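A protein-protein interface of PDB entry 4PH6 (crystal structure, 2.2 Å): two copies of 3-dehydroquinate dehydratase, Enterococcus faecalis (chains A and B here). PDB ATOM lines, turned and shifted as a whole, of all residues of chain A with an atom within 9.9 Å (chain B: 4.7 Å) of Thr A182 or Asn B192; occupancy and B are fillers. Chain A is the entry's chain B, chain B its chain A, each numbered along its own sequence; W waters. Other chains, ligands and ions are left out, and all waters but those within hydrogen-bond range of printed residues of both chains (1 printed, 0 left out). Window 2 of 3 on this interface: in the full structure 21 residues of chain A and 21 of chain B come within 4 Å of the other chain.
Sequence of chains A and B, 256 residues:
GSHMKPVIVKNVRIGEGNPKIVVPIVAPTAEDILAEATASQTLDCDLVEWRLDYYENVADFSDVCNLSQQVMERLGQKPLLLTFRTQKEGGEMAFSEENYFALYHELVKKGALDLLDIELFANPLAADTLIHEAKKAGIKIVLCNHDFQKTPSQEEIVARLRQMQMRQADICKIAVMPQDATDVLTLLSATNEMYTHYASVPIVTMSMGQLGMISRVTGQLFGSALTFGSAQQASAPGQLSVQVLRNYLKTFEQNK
3 positions are printed for both chains.
Thr A182 touches just one residue of chain B: Asn B192 (2.9 Å). Printed residues of chain B within 4 Å of Leu A185: Leu B188, Ser B189, Asn B192 and Phe B222. Of the printed residues of chain B, Leu A211 touches Leu B221. No residue of chain A comes within 4 Å of Ala B190. Of chain A, only Ala A181 (3.6 Å), Thr A182 (2.9 Å) and Leu A185 (3.8 Å) come within 4 Å of Asn B192. Of the printed residues of chain A, Leu B221 touches Ala A181 (3.3 Å), Leu A211 (3.4 Å) and Ile A214 (3.7 Å). Of the printed residues of chain A, Phe B222 touches Ala A181 (3.8 Å), Leu A185 (3.5 Å) and Ile A214 (3.7 Å). The nearest printed residue of chain B that does not touch Thr A182 is Thr B196 (5.4 Å). The nearest residue of chain A that does not touch Asn B192 is Asp A183 (6.4 Å). The nearest printed residue of chain B that does not touch Ala A181 is Thr B196 (6.5 Å).
The side-chain amide nitrogen of Asn B192 lies within hydrogen-bond range of the side-chain hydroxyl of Thr A182, at 2.9 Å.
Water W1 bridges OG1 of Thr A182 (2.5 Å) and OD1 of Asn B192 (3.5 Å).
Of the 24 printed residues of chain A, 5 touch a printed residue of chain B.
Asn B192 touches Ala A181. O of Leu B221 touches CB of Ala A181, 3.3 Å away. O of Ala A181 touches CE2 of Phe B222, at 3.8 Å. CD2 of Leu A185 touches CB of Leu B188, at 3.8 Å. CD1 of Leu A185 touches OG of Ser B189, 3.8 Å away. Asn B192 touches Leu A185 (CB to CD1, 3.8 Å). CG of Leu A185 touches CE2 of Phe B222, at 3.5 Å. Leu A211 touches Leu B221 (O to CD2, 3.4 Å). Leu B221 touches Ile A214. Ile A214 touches Phe B222 (CD1 to CZ, 3.7 Å).
O of Asn B192 is in hydrogen-bond range of OG1 of Thr B196. N of Thr A182 sits close to OD1 of Asp A180 (3.3 Å). The backbone carbonyl oxygen of Thr A182 lies within hydrogen-bond range of the side-chain hydroxyl of Thr A186, 2.8 Å away. The side-chain hydroxyl (OG) of Ser A189 sits at hydrogen-bond distance from the backbone carbonyl oxygen (O) of Leu A185, 2.9 Å away.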
ATOM      1  N   THR A 151     -24.908 -28.346   7.189  1.00  0.00           N
ATOM      2  CA  THR A 151     -24.136 -29.558   6.980  1.00  0.00           C
ATOM      3  C   THR A 151     -23.621 -30.054   8.334  1.00  0.00           C
ATOM      4  O   THR A 151     -22.831 -29.367   8.987  1.00  0.00           O
ATOM      5  CB  THR A 151     -22.955 -29.327   6.015  1.00  0.00           C
ATOM      6  OG1 THR A 151     -23.410 -28.634   4.842  1.00  0.00           O
ATOM      7  CG2 THR A 151     -22.344 -30.667   5.605  1.00  0.00           C
ATOM      8  N   PRO A 152     -24.089 -31.232   8.774  1.00  0.00           N
ATOM      9  CA  PRO A 152     -23.625 -31.844  10.031  1.00  0.00           C
ATOM     10  C   PRO A 152     -22.136 -32.192   9.934  1.00  0.00           C
ATOM     11  O   PRO A 152     -21.575 -32.130   8.845  1.00  0.00           O
ATOM     12  CB  PRO A 152     -24.473 -33.129  10.156  1.00  0.00           C
ATOM     13  CG  PRO A 152     -25.606 -32.973   9.175  1.00  0.00           C
ATOM     14  CD  PRO A 152     -25.062 -32.085   8.070  1.00  0.00           C
ATOM     15  N   SER A 153     -21.510 -32.572  11.040  1.00  0.00           N
ATOM     16  CA  SER A 153     -20.086 -32.908  11.014  1.00  0.00           C
ATOM     17  C   SER A 153     -19.828 -34.111  10.095  1.00  0.00           C
ATOM     18  O   SER A 153     -20.743 -34.879   9.796  1.00  0.00           O
ATOM     19  CB  SER A 153     -19.568 -33.205  12.421  1.00  0.00           C
ATOM     20  OG  SER A 153     -19.998 -34.487  12.846  1.00  0.00           O
ATOM     21  N   GLN A 154     -18.589 -34.263   9.642  1.00  0.00           N
ATOM     22  CA  GLN A 154     -18.227 -35.389   8.793  1.00  0.00           C
ATOM     23  C   GLN A 154     -18.615 -36.720   9.460  1.00  0.00           C
ATOM     24  O   GLN A 154     -19.177 -37.615   8.812  1.00  0.00           O
ATOM     25  CB  GLN A 154     -16.730 -35.359   8.472  1.00  0.00           C
ATOM     26  CG  GLN A 154     -16.210 -36.679   7.929  1.00  0.00           C
ATOM     27  CD  GLN A 154     -14.802 -36.589   7.375  1.00  0.00           C
ATOM     28  OE1 GLN A 154     -14.263 -35.499   7.191  1.00  0.00           O
ATOM     29  NE2 GLN A 154     -14.205 -37.737   7.086  1.00  0.00           N
ATOM     30  N   ILE A 157     -22.461 -37.403   9.409  1.00  0.00           N
ATOM     31  CA  ILE A 157     -22.890 -37.800   8.070  1.00  0.00           C
ATOM     32  C   ILE A 157     -22.566 -39.273   7.856  1.00  0.00           C
ATOM     33  O   ILE A 157     -23.438 -40.050   7.466  1.00  0.00           O
ATOM     34  CB  ILE A 157     -22.236 -36.914   6.980  1.00  0.00           C
ATOM     35  CG1 ILE A 157     -22.717 -35.463   7.154  1.00  0.00           C
ATOM     36  CG2 ILE A 157     -22.557 -37.429   5.574  1.00  0.00           C
ATOM     37  CD1 ILE A 157     -21.999 -34.428   6.296  1.00  0.00           C
ATOM     38  N   VAL A 176     -27.087 -32.734   2.112  1.00  0.00           N
ATOM     39  CA  VAL A 176     -26.870 -31.731   3.157  1.00  0.00           C
ATOM     40  C   VAL A 176     -26.720 -30.347   2.525  1.00  0.00           C
ATOM     41  O   VAL A 176     -26.474 -30.244   1.333  1.00  0.00           O
ATOM     42  CB  VAL A 176     -25.631 -32.065   4.010  1.00  0.00           C
ATOM     43  CG1 VAL A 176     -25.854 -33.366   4.805  1.00  0.00           C
ATOM     44  CG2 VAL A 176     -24.386 -32.172   3.123  1.00  0.00           C
ATOM     45  N   MET A 177     -26.897 -29.283   3.306  1.00  0.00           N
ATOM     46  CA  MET A 177     -26.820 -27.939   2.745  1.00  0.00           C
ATOM     47  C   MET A 177     -25.571 -27.192   3.192  1.00  0.00           C
ATOM     48  O   MET A 177     -25.422 -26.885   4.372  1.00  0.00           O
ATOM     49  CB  MET A 177     -28.055 -27.110   3.114  1.00  0.00           C
ATOM     50  CG  MET A 177     -27.998 -25.669   2.580  1.00  0.00           C
ATOM     51  SD  MET A 177     -28.129 -25.559   0.769  1.00  0.00           S
ATOM     52  CE  MET A 177     -29.887 -25.742   0.507  1.00  0.00           C
ATOM     53  N   PRO A 178     -24.667 -26.889   2.245  1.00  0.00           N
ATOM     54  CA  PRO A 178     -23.449 -26.151   2.580  1.00  0.00           C
ATOM     55  C   PRO A 178     -23.725 -24.681   2.789  1.00  0.00           C
ATOM     56  O   PRO A 178     -24.576 -24.109   2.108  1.00  0.00           O
ATOM     57  CB  PRO A 178     -22.572 -26.353   1.350  1.00  0.00           C
ATOM     58  CG  PRO A 178     -23.527 -26.416   0.260  1.00  0.00           C
ATOM     59  CD  PRO A 178     -24.698 -27.217   0.813  1.00  0.00           C
ATOM     60  N   GLN A 179     -23.002 -24.074   3.719  1.00  0.00           N
ATOM     61  CA  GLN A 179     -23.065 -22.634   3.895  1.00  0.00           C
ATOM     62  C   GLN A 179     -21.752 -21.995   3.433  1.00  0.00           C
ATOM     63  O   GLN A 179     -21.667 -20.775   3.275  1.00  0.00           O
ATOM     64  CB  GLN A 179     -23.382 -22.294   5.352  1.00  0.00           C
ATOM     65  CG  GLN A 179     -24.714 -22.910   5.824  1.00  0.00           C
ATOM     66  CD  GLN A 179     -25.065 -22.566   7.257  1.00  0.00           C
ATOM     67  OE1 GLN A 179     -24.951 -23.402   8.160  1.00  0.00           O
ATOM     68  NE2 GLN A 179     -25.497 -21.327   7.477  1.00  0.00           N
ATOM     69  N   ASP A 180     -20.735 -22.822   3.203  1.00  0.00           N
ATOM     70  CA  ASP A 180     -19.449 -22.343   2.683  1.00  0.00           C
ATOM     71  C   ASP A 180     -18.675 -23.505   2.053  1.00  0.00           C
ATOM     72  O   ASP A 180     -19.187 -24.631   2.009  1.00  0.00           O
ATOM     73  CB  ASP A 180     -18.611 -21.670   3.788  1.00  0.00           C
ATOM     74  CG  ASP A 180     -18.334 -22.582   4.976  1.00  0.00           C
ATOM     75  OD1 ASP A 180     -18.435 -23.822   4.854  1.00  0.00           O
ATOM     76  OD2 ASP A 180     -17.983 -22.051   6.048  1.00  0.00           O
ATOM     77  N   ALA A 181     -17.453 -23.243   1.590  1.00  0.00           N
ATOM     78  CA  ALA A 181     -16.689 -24.244   0.831  1.00  0.00           C
ATOM     79  C   ALA A 181     -16.234 -25.388   1.723  1.00  0.00           C
ATOM     80  O   ALA A 181     -16.134 -26.541   1.285  1.00  0.00           O
ATOM     81  CB  ALA A 181     -15.489 -23.602   0.143  1.00  0.00           C
ATOM     82  N   THR A 182     -15.962 -25.059   2.981  1.00  0.00           N
ATOM     83  CA  THR A 182     -15.591 -26.060   3.970  1.00  0.00           C
ATOM     84  C   THR A 182     -16.675 -27.134   4.110  1.00  0.00           C
ATOM     85  O   THR A 182     -16.379 -28.314   4.255  1.00  0.00           O
ATOM     86  CB  THR A 182     -15.330 -25.404   5.329  1.00  0.00           C
ATOM     87  OG1 THR A 182     -14.310 -24.423   5.174  1.00  0.00           O
ATOM     88  CG2 THR A 182     -14.857 -26.420   6.344  1.00  0.00           C
ATOM     89  N   ASP A 183     -17.935 -26.723   4.046  1.00  0.00           N
ATOM     90  CA  ASP A 183     -19.041 -27.661   4.199  1.00  0.00           C
ATOM     91  C   ASP A 183     -19.109 -28.653   3.046  1.00  0.00           C
ATOM     92  O   ASP A 183     -19.487 -29.806   3.245  1.00  0.00           O
ATOM     93  CB  ASP A 183     -20.367 -26.913   4.323  1.00  0.00           C
ATOM     94  CG  ASP A 183     -20.610 -26.391   5.720  1.00  0.00           C
ATOM     95  OD1 ASP A 183     -19.915 -26.840   6.657  1.00  0.00           O
ATOM     96  OD2 ASP A 183     -21.507 -25.545   5.888  1.00  0.00           O
ATOM     97  N   VAL A 184     -18.730 -28.207   1.847  1.00  0.00           N
ATOM     98  CA  VAL A 184     -18.768 -29.070   0.673  1.00  0.00           C
ATOM     99  C   VAL A 184     -17.714 -30.165   0.811  1.00  0.00           C
ATOM    100  O   VAL A 184     -17.985 -31.337   0.563  1.00  0.00           O
ATOM    101  CB  VAL A 184     -18.529 -28.282  -0.638  1.00  0.00           C
ATOM    102  CG1 VAL A 184     -18.718 -29.193  -1.850  1.00  0.00           C
ATOM    103  CG2 VAL A 184     -19.462 -27.077  -0.707  1.00  0.00           C
ATOM    104  N   LEU A 185     -16.513 -29.769   1.218  1.00  0.00           N
ATOM    105  CA  LEU A 185     -15.427 -30.698   1.507  1.00  0.00           C
ATOM    106  C   LEU A 185     -15.820 -31.728   2.563  1.00  0.00           C
ATOM    107  O   LEU A 185     -15.529 -32.910   2.429  1.00  0.00           O
ATOM    108  CB  LEU A 185     -14.194 -29.931   1.977  1.00  0.00           C
ATOM    109  CG  LEU A 185     -13.430 -29.222   0.866  1.00  0.00           C
ATOM    110  CD1 LEU A 185     -12.434 -28.214   1.442  1.00  0.00           C
ATOM    111  CD2 LEU A 185     -12.732 -30.264   0.010  1.00  0.00           C
ATOM    112  N   THR A 186     -16.461 -31.253   3.622  1.00  0.00           N
ATOM    113  CA  THR A 186     -16.973 -32.114   4.672  1.00  0.00           C
ATOM    114  C   THR A 186     -17.844 -33.237   4.100  1.00  0.00           C
ATOM    115  O   THR A 186     -17.663 -34.412   4.438  1.00  0.00           O
ATOM    116  CB  THR A 186     -17.781 -31.296   5.691  1.00  0.00           C
ATOM    117  OG1 THR A 186     -16.943 -30.267   6.231  1.00  0.00           O
ATOM    118  CG2 THR A 186     -18.299 -32.179   6.810  1.00  0.00           C
ATOM    119  N   LEU A 187     -18.764 -32.870   3.214  1.00  0.00           N
ATOM    120  CA  LEU A 187     -19.643 -33.838   2.563  1.00  0.00           C
ATOM    121  C   LEU A 187     -18.850 -34.766   1.646  1.00  0.00           C
ATOM    122  O   LEU A 187     -19.023 -35.985   1.681  1.00  0.00           O
ATOM    123  CB  LEU A 187     -20.741 -33.111   1.787  1.00  0.00           C
ATOM    124  CG  LEU A 187     -21.848 -33.911   1.077  1.00  0.00           C
ATOM    125  CD1 LEU A 187     -21.427 -34.343  -0.344  1.00  0.00           C
ATOM    126  CD2 LEU A 187     -22.321 -35.111   1.914  1.00  0.00           C
ATOM    127  N   LEU A 188     -17.976 -34.193   0.826  1.00  0.00           N
ATOM    128  CA  LEU A 188     -17.162 -35.003  -0.076  1.00  0.00           C
ATOM    129  C   LEU A 188     -16.290 -35.978   0.724  1.00  0.00           C
ATOM    130  O   LEU A 188     -16.206 -37.150   0.376  1.00  0.00           O
ATOM    131  CB  LEU A 188     -16.304 -34.114  -0.983  1.00  0.00           C
ATOM    132  CG  LEU A 188     -17.058 -33.241  -1.999  1.00  0.00           C
ATOM    133  CD1 LEU A 188     -16.120 -32.289  -2.698  1.00  0.00           C
ATOM    134  CD2 LEU A 188     -17.793 -34.101  -3.042  1.00  0.00           C
ATOM    135  N   SER A 189     -15.687 -35.500   1.812  1.00  0.00           N
ATOM    136  CA  SER A 189     -14.877 -36.348   2.696  1.00  0.00           C
ATOM    137  C   SER A 189     -15.684 -37.420   3.417  1.00  0.00           C
ATOM    138  O   SER A 189     -15.224 -38.543   3.584  1.00  0.00           O
ATOM    139  CB  SER A 189     -14.155 -35.508   3.751  1.00  0.00           C
ATOM    140  OG  SER A 189     -13.303 -34.575   3.134  1.00  0.00           O
ATOM    141  N   ALA A 190     -16.869 -37.055   3.887  1.00  0.00           N
ATOM    142  CA  ALA A 190     -17.753 -38.030   4.506  1.00  0.00           C
ATOM    143  C   ALA A 190     -18.060 -39.138   3.510  1.00  0.00           C
ATOM    144  O   ALA A 190     -18.005 -40.312   3.854  1.00  0.00           O
ATOM    145  CB  ALA A 190     -19.028 -37.374   4.992  1.00  0.00           C
ATOM    146  N   SER A 207     -24.005 -32.396  -1.738  1.00  0.00           N
ATOM    147  CA  SER A 207     -24.024 -31.097  -1.108  1.00  0.00           C
ATOM    148  C   SER A 207     -24.892 -30.180  -1.967  1.00  0.00           C
ATOM    149  O   SER A 207     -24.593 -29.956  -3.151  1.00  0.00           O
ATOM    150  CB  SER A 207     -22.602 -30.556  -0.967  1.00  0.00           C
ATOM    151  OG  SER A 207     -22.577 -29.373  -0.204  1.00  0.00           O
ATOM    152  N   LEU A 211     -23.031 -23.866  -4.245  1.00  0.00           N
ATOM    153  CA  LEU A 211     -21.752 -24.207  -3.608  1.00  0.00           C
ATOM    154  C   LEU A 211     -21.357 -25.682  -3.767  1.00  0.00           C
ATOM    155  O   LEU A 211     -20.194 -25.989  -4.032  1.00  0.00           O
ATOM    156  CB  LEU A 211     -21.779 -23.865  -2.111  1.00  0.00           C
ATOM    157  CG  LEU A 211     -21.716 -22.403  -1.667  1.00  0.00           C
ATOM    158  CD1 LEU A 211     -21.815 -22.274  -0.160  1.00  0.00           C
ATOM    159  CD2 LEU A 211     -20.457 -21.747  -2.168  1.00  0.00           C
ATOM    160  N   GLY A 212     -22.321 -26.588  -3.595  1.00  0.00           N
ATOM    161  CA  GLY A 212     -22.032 -28.010  -3.596  1.00  0.00           C
ATOM    162  C   GLY A 212     -22.238 -28.697  -4.935  1.00  0.00           C
ATOM    163  O   GLY A 212     -22.252 -29.930  -5.011  1.00  0.00           O
ATOM    164  N   ILE A 214     -20.376 -29.302  -7.440  1.00  0.00           N
ATOM    165  CA  ILE A 214     -19.326 -30.262  -7.781  1.00  0.00           C
ATOM    166  C   ILE A 214     -19.579 -31.679  -7.282  1.00  0.00           C
ATOM    167  O   ILE A 214     -19.103 -32.631  -7.885  1.00  0.00           O
ATOM    168  CB  ILE A 214     -17.966 -29.847  -7.214  1.00  0.00           C
ATOM    169  CG1 ILE A 214     -18.092 -29.585  -5.712  1.00  0.00           C
ATOM    170  CG2 ILE A 214     -17.439 -28.651  -7.954  1.00  0.00           C
ATOM    171  CD1 ILE A 214     -16.792 -29.310  -5.036  1.00  0.00           C
ATOM    172  N   LEU B 188      -7.458 -30.299  -2.116  1.00  0.00           N
ATOM    173  CA  LEU B 188      -8.566 -29.340  -2.086  1.00  0.00           C
ATOM    174  C   LEU B 188      -8.701 -28.666  -0.713  1.00  0.00           C
ATOM    175  O   LEU B 188      -8.876 -27.457  -0.636  1.00  0.00           O
ATOM    176  CB  LEU B 188      -9.881 -30.020  -2.481  1.00  0.00           C
ATOM    177  CG  LEU B 188      -9.966 -30.475  -3.939  1.00  0.00           C
ATOM    178  CD1 LEU B 188     -11.226 -31.271  -4.213  1.00  0.00           C
ATOM    179  CD2 LEU B 188      -9.896 -29.266  -4.851  1.00  0.00           C
ATOM    180  N   SER B 189      -8.602 -29.446   0.360  1.00  0.00           N
ATOM    181  CA  SER B 189      -8.653 -28.912   1.731  1.00  0.00           C
ATOM    182  C   SER B 189      -7.486 -27.988   2.079  1.00  0.00           C
ATOM    183  O   SER B 189      -7.663 -26.962   2.731  1.00  0.00           O
ATOM    184  CB  SER B 189      -8.677 -30.050   2.747  1.00  0.00           C
ATOM    185  OG  SER B 189      -9.912 -30.721   2.710  1.00  0.00           O
ATOM    186  N   ALA B 190      -6.289 -28.398   1.674  1.00  0.00           N
ATOM    187  CA  ALA B 190      -5.088 -27.589   1.842  1.00  0.00           C
ATOM    188  C   ALA B 190      -5.280 -26.230   1.177  1.00  0.00           C
ATOM    189  O   ALA B 190      -4.937 -25.178   1.742  1.00  0.00           O
ATOM    190  CB  ALA B 190      -3.879 -28.307   1.257  1.00  0.00           C
ATOM    191  N   THR B 191      -5.846 -26.267  -0.018  1.00  0.00           N
ATOM    192  CA  THR B 191      -6.179 -25.052  -0.761  1.00  0.00           C
ATOM    193  C   THR B 191      -7.164 -24.187   0.029  1.00  0.00           C
ATOM    194  O   THR B 191      -6.948 -22.985   0.172  1.00  0.00           O
ATOM    195  CB  THR B 191      -6.792 -25.374  -2.153  1.00  0.00           C
ATOM    196  OG1 THR B 191      -5.867 -26.150  -2.923  1.00  0.00           O
ATOM    197  CG2 THR B 191      -7.144 -24.082  -2.919  1.00  0.00           C
ATOM    198  N   ASN B 192      -8.234 -24.796   0.539  1.00  0.00           N
ATOM    199  CA  ASN B 192      -9.248 -24.042   1.285  1.00  0.00           C
ATOM    200  C   ASN B 192      -8.699 -23.429   2.586  1.00  0.00           C
ATOM    201  O   ASN B 192      -8.900 -22.251   2.839  1.00  0.00           O
ATOM    202  CB  ASN B 192     -10.469 -24.921   1.607  1.00  0.00           C
ATOM    203  CG  ASN B 192     -11.611 -24.122   2.254  1.00  0.00           C
ATOM    204  OD1 ASN B 192     -12.186 -23.217   1.636  1.00  0.00           O
ATOM    205  ND2 ASN B 192     -11.944 -24.459   3.496  1.00  0.00           N
ATOM    206  N   GLU B 193      -8.008 -24.229   3.395  1.00  0.00           N
ATOM    207  CA  GLU B 193      -7.386 -23.734   4.626  1.00  0.00           C
ATOM    208  C   GLU B 193      -6.405 -22.578   4.375  1.00  0.00           C
ATOM    209  O   GLU B 193      -6.491 -21.536   5.023  1.00  0.00           O
ATOM    210  CB  GLU B 193      -6.661 -24.863   5.351  1.00  0.00           C
ATOM    211  CG  GLU B 193      -5.829 -24.390   6.551  1.00  0.00           C
ATOM    212  CD  GLU B 193      -5.108 -25.530   7.240  1.00  0.00           C
ATOM    213  OE1 GLU B 193      -5.306 -26.695   6.834  1.00  0.00           O
ATOM    214  OE2 GLU B 193      -4.347 -25.266   8.199  1.00  0.00           O
ATOM    215  N   MET B 194      -5.477 -22.764   3.437  1.00  0.00           N
ATOM    216  CA  MET B 194      -4.521 -21.707   3.090  1.00  0.00           C
ATOM    217  C   MET B 194      -5.230 -20.411   2.722  1.00  0.00           C
ATOM    218  O   MET B 194      -4.914 -19.336   3.245  1.00  0.00           O
ATOM    219  CB  MET B 194      -3.617 -22.136   1.924  1.00  0.00           C
ATOM    220  CG  MET B 194      -2.626 -21.058   1.477  1.00  0.00           C
ATOM    221  SD  MET B 194      -1.367 -20.713   2.736  1.00  0.00           S
ATOM    222  CE  MET B 194      -0.668 -19.184   2.127  1.00  0.00           C
ATOM    223  N   TYR B 195      -6.193 -20.520   1.821  1.00  0.00           N
ATOM    224  CA  TYR B 195      -6.905 -19.365   1.299  1.00  0.00           C
ATOM    225  C   TYR B 195      -7.703 -18.642   2.374  1.00  0.00           C
ATOM    226  O   TYR B 195      -7.739 -17.414   2.409  1.00  0.00           O
ATOM    227  CB  TYR B 195      -7.838 -19.799   0.167  1.00  0.00           C
ATOM    228  CG  TYR B 195      -8.683 -18.687  -0.409  1.00  0.00           C
ATOM    229  CD1 TYR B 195      -8.200 -17.866  -1.425  1.00  0.00           C
ATOM    230  CD2 TYR B 195      -9.967 -18.459   0.061  1.00  0.00           C
ATOM    231  CE1 TYR B 195      -8.976 -16.861  -1.955  1.00  0.00           C
ATOM    232  CE2 TYR B 195     -10.750 -17.444  -0.459  1.00  0.00           C
ATOM    233  CZ  TYR B 195     -10.252 -16.653  -1.465  1.00  0.00           C
ATOM    234  OH  TYR B 195     -11.045 -15.655  -1.979  1.00  0.00           O
ATOM    235  N   THR B 196      -8.354 -19.393   3.256  1.00  0.00           N
ATOM    236  CA  THR B 196      -9.226 -18.746   4.221  1.00  0.00           C
ATOM    237  C   THR B 196      -8.422 -18.148   5.389  1.00  0.00           C
ATOM    238  O   THR B 196      -8.792 -17.112   5.932  1.00  0.00           O
ATOM    239  CB  THR B 196     -10.309 -19.723   4.763  1.00  0.00           C
ATOM    240  OG1 THR B 196      -9.692 -20.838   5.410  1.00  0.00           O
ATOM    241  CG2 THR B 196     -11.178 -20.243   3.626  1.00  0.00           C
ATOM    242  N   LEU B 221     -14.377 -21.909  -5.905  1.00  0.00           N
ATOM    243  CA  LEU B 221     -14.931 -22.397  -4.655  1.00  0.00           C
ATOM    244  C   LEU B 221     -13.898 -22.469  -3.536  1.00  0.00           C
ATOM    245  O   LEU B 221     -14.175 -22.060  -2.404  1.00  0.00           O
ATOM    246  CB  LEU B 221     -15.556 -23.775  -4.864  1.00  0.00           C
ATOM    247  CG  LEU B 221     -16.162 -24.441  -3.634  1.00  0.00           C
ATOM    248  CD1 LEU B 221     -17.199 -23.528  -2.997  1.00  0.00           C
ATOM    249  CD2 LEU B 221     -16.786 -25.769  -4.034  1.00  0.00           C
ATOM    250  N   PHE B 222     -12.712 -22.987  -3.845  1.00  0.00           N
ATOM    251  CA  PHE B 222     -11.742 -23.308  -2.806  1.00  0.00           C
ATOM    252  C   PHE B 222     -10.590 -22.299  -2.727  1.00  0.00           C
ATOM    253  O   PHE B 222      -9.809 -22.330  -1.787  1.00  0.00           O
ATOM    254  CB  PHE B 222     -11.187 -24.722  -3.009  1.00  0.00           C
ATOM    255  CG  PHE B 222     -12.231 -25.798  -2.947  1.00  0.00           C
ATOM    256  CD1 PHE B 222     -12.436 -26.642  -4.018  1.00  0.00           C
ATOM    257  CD2 PHE B 222     -13.012 -25.963  -1.818  1.00  0.00           C
ATOM    258  CE1 PHE B 222     -13.408 -27.651  -3.964  1.00  0.00           C
ATOM    259  CE2 PHE B 222     -13.979 -26.956  -1.758  1.00  0.00           C
ATOM    260  CZ  PHE B 222     -14.179 -27.801  -2.832  1.00  0.00           C
HETATM  261  O   HOH W   1     -14.747 -22.408   3.846  1.00  0.00           O
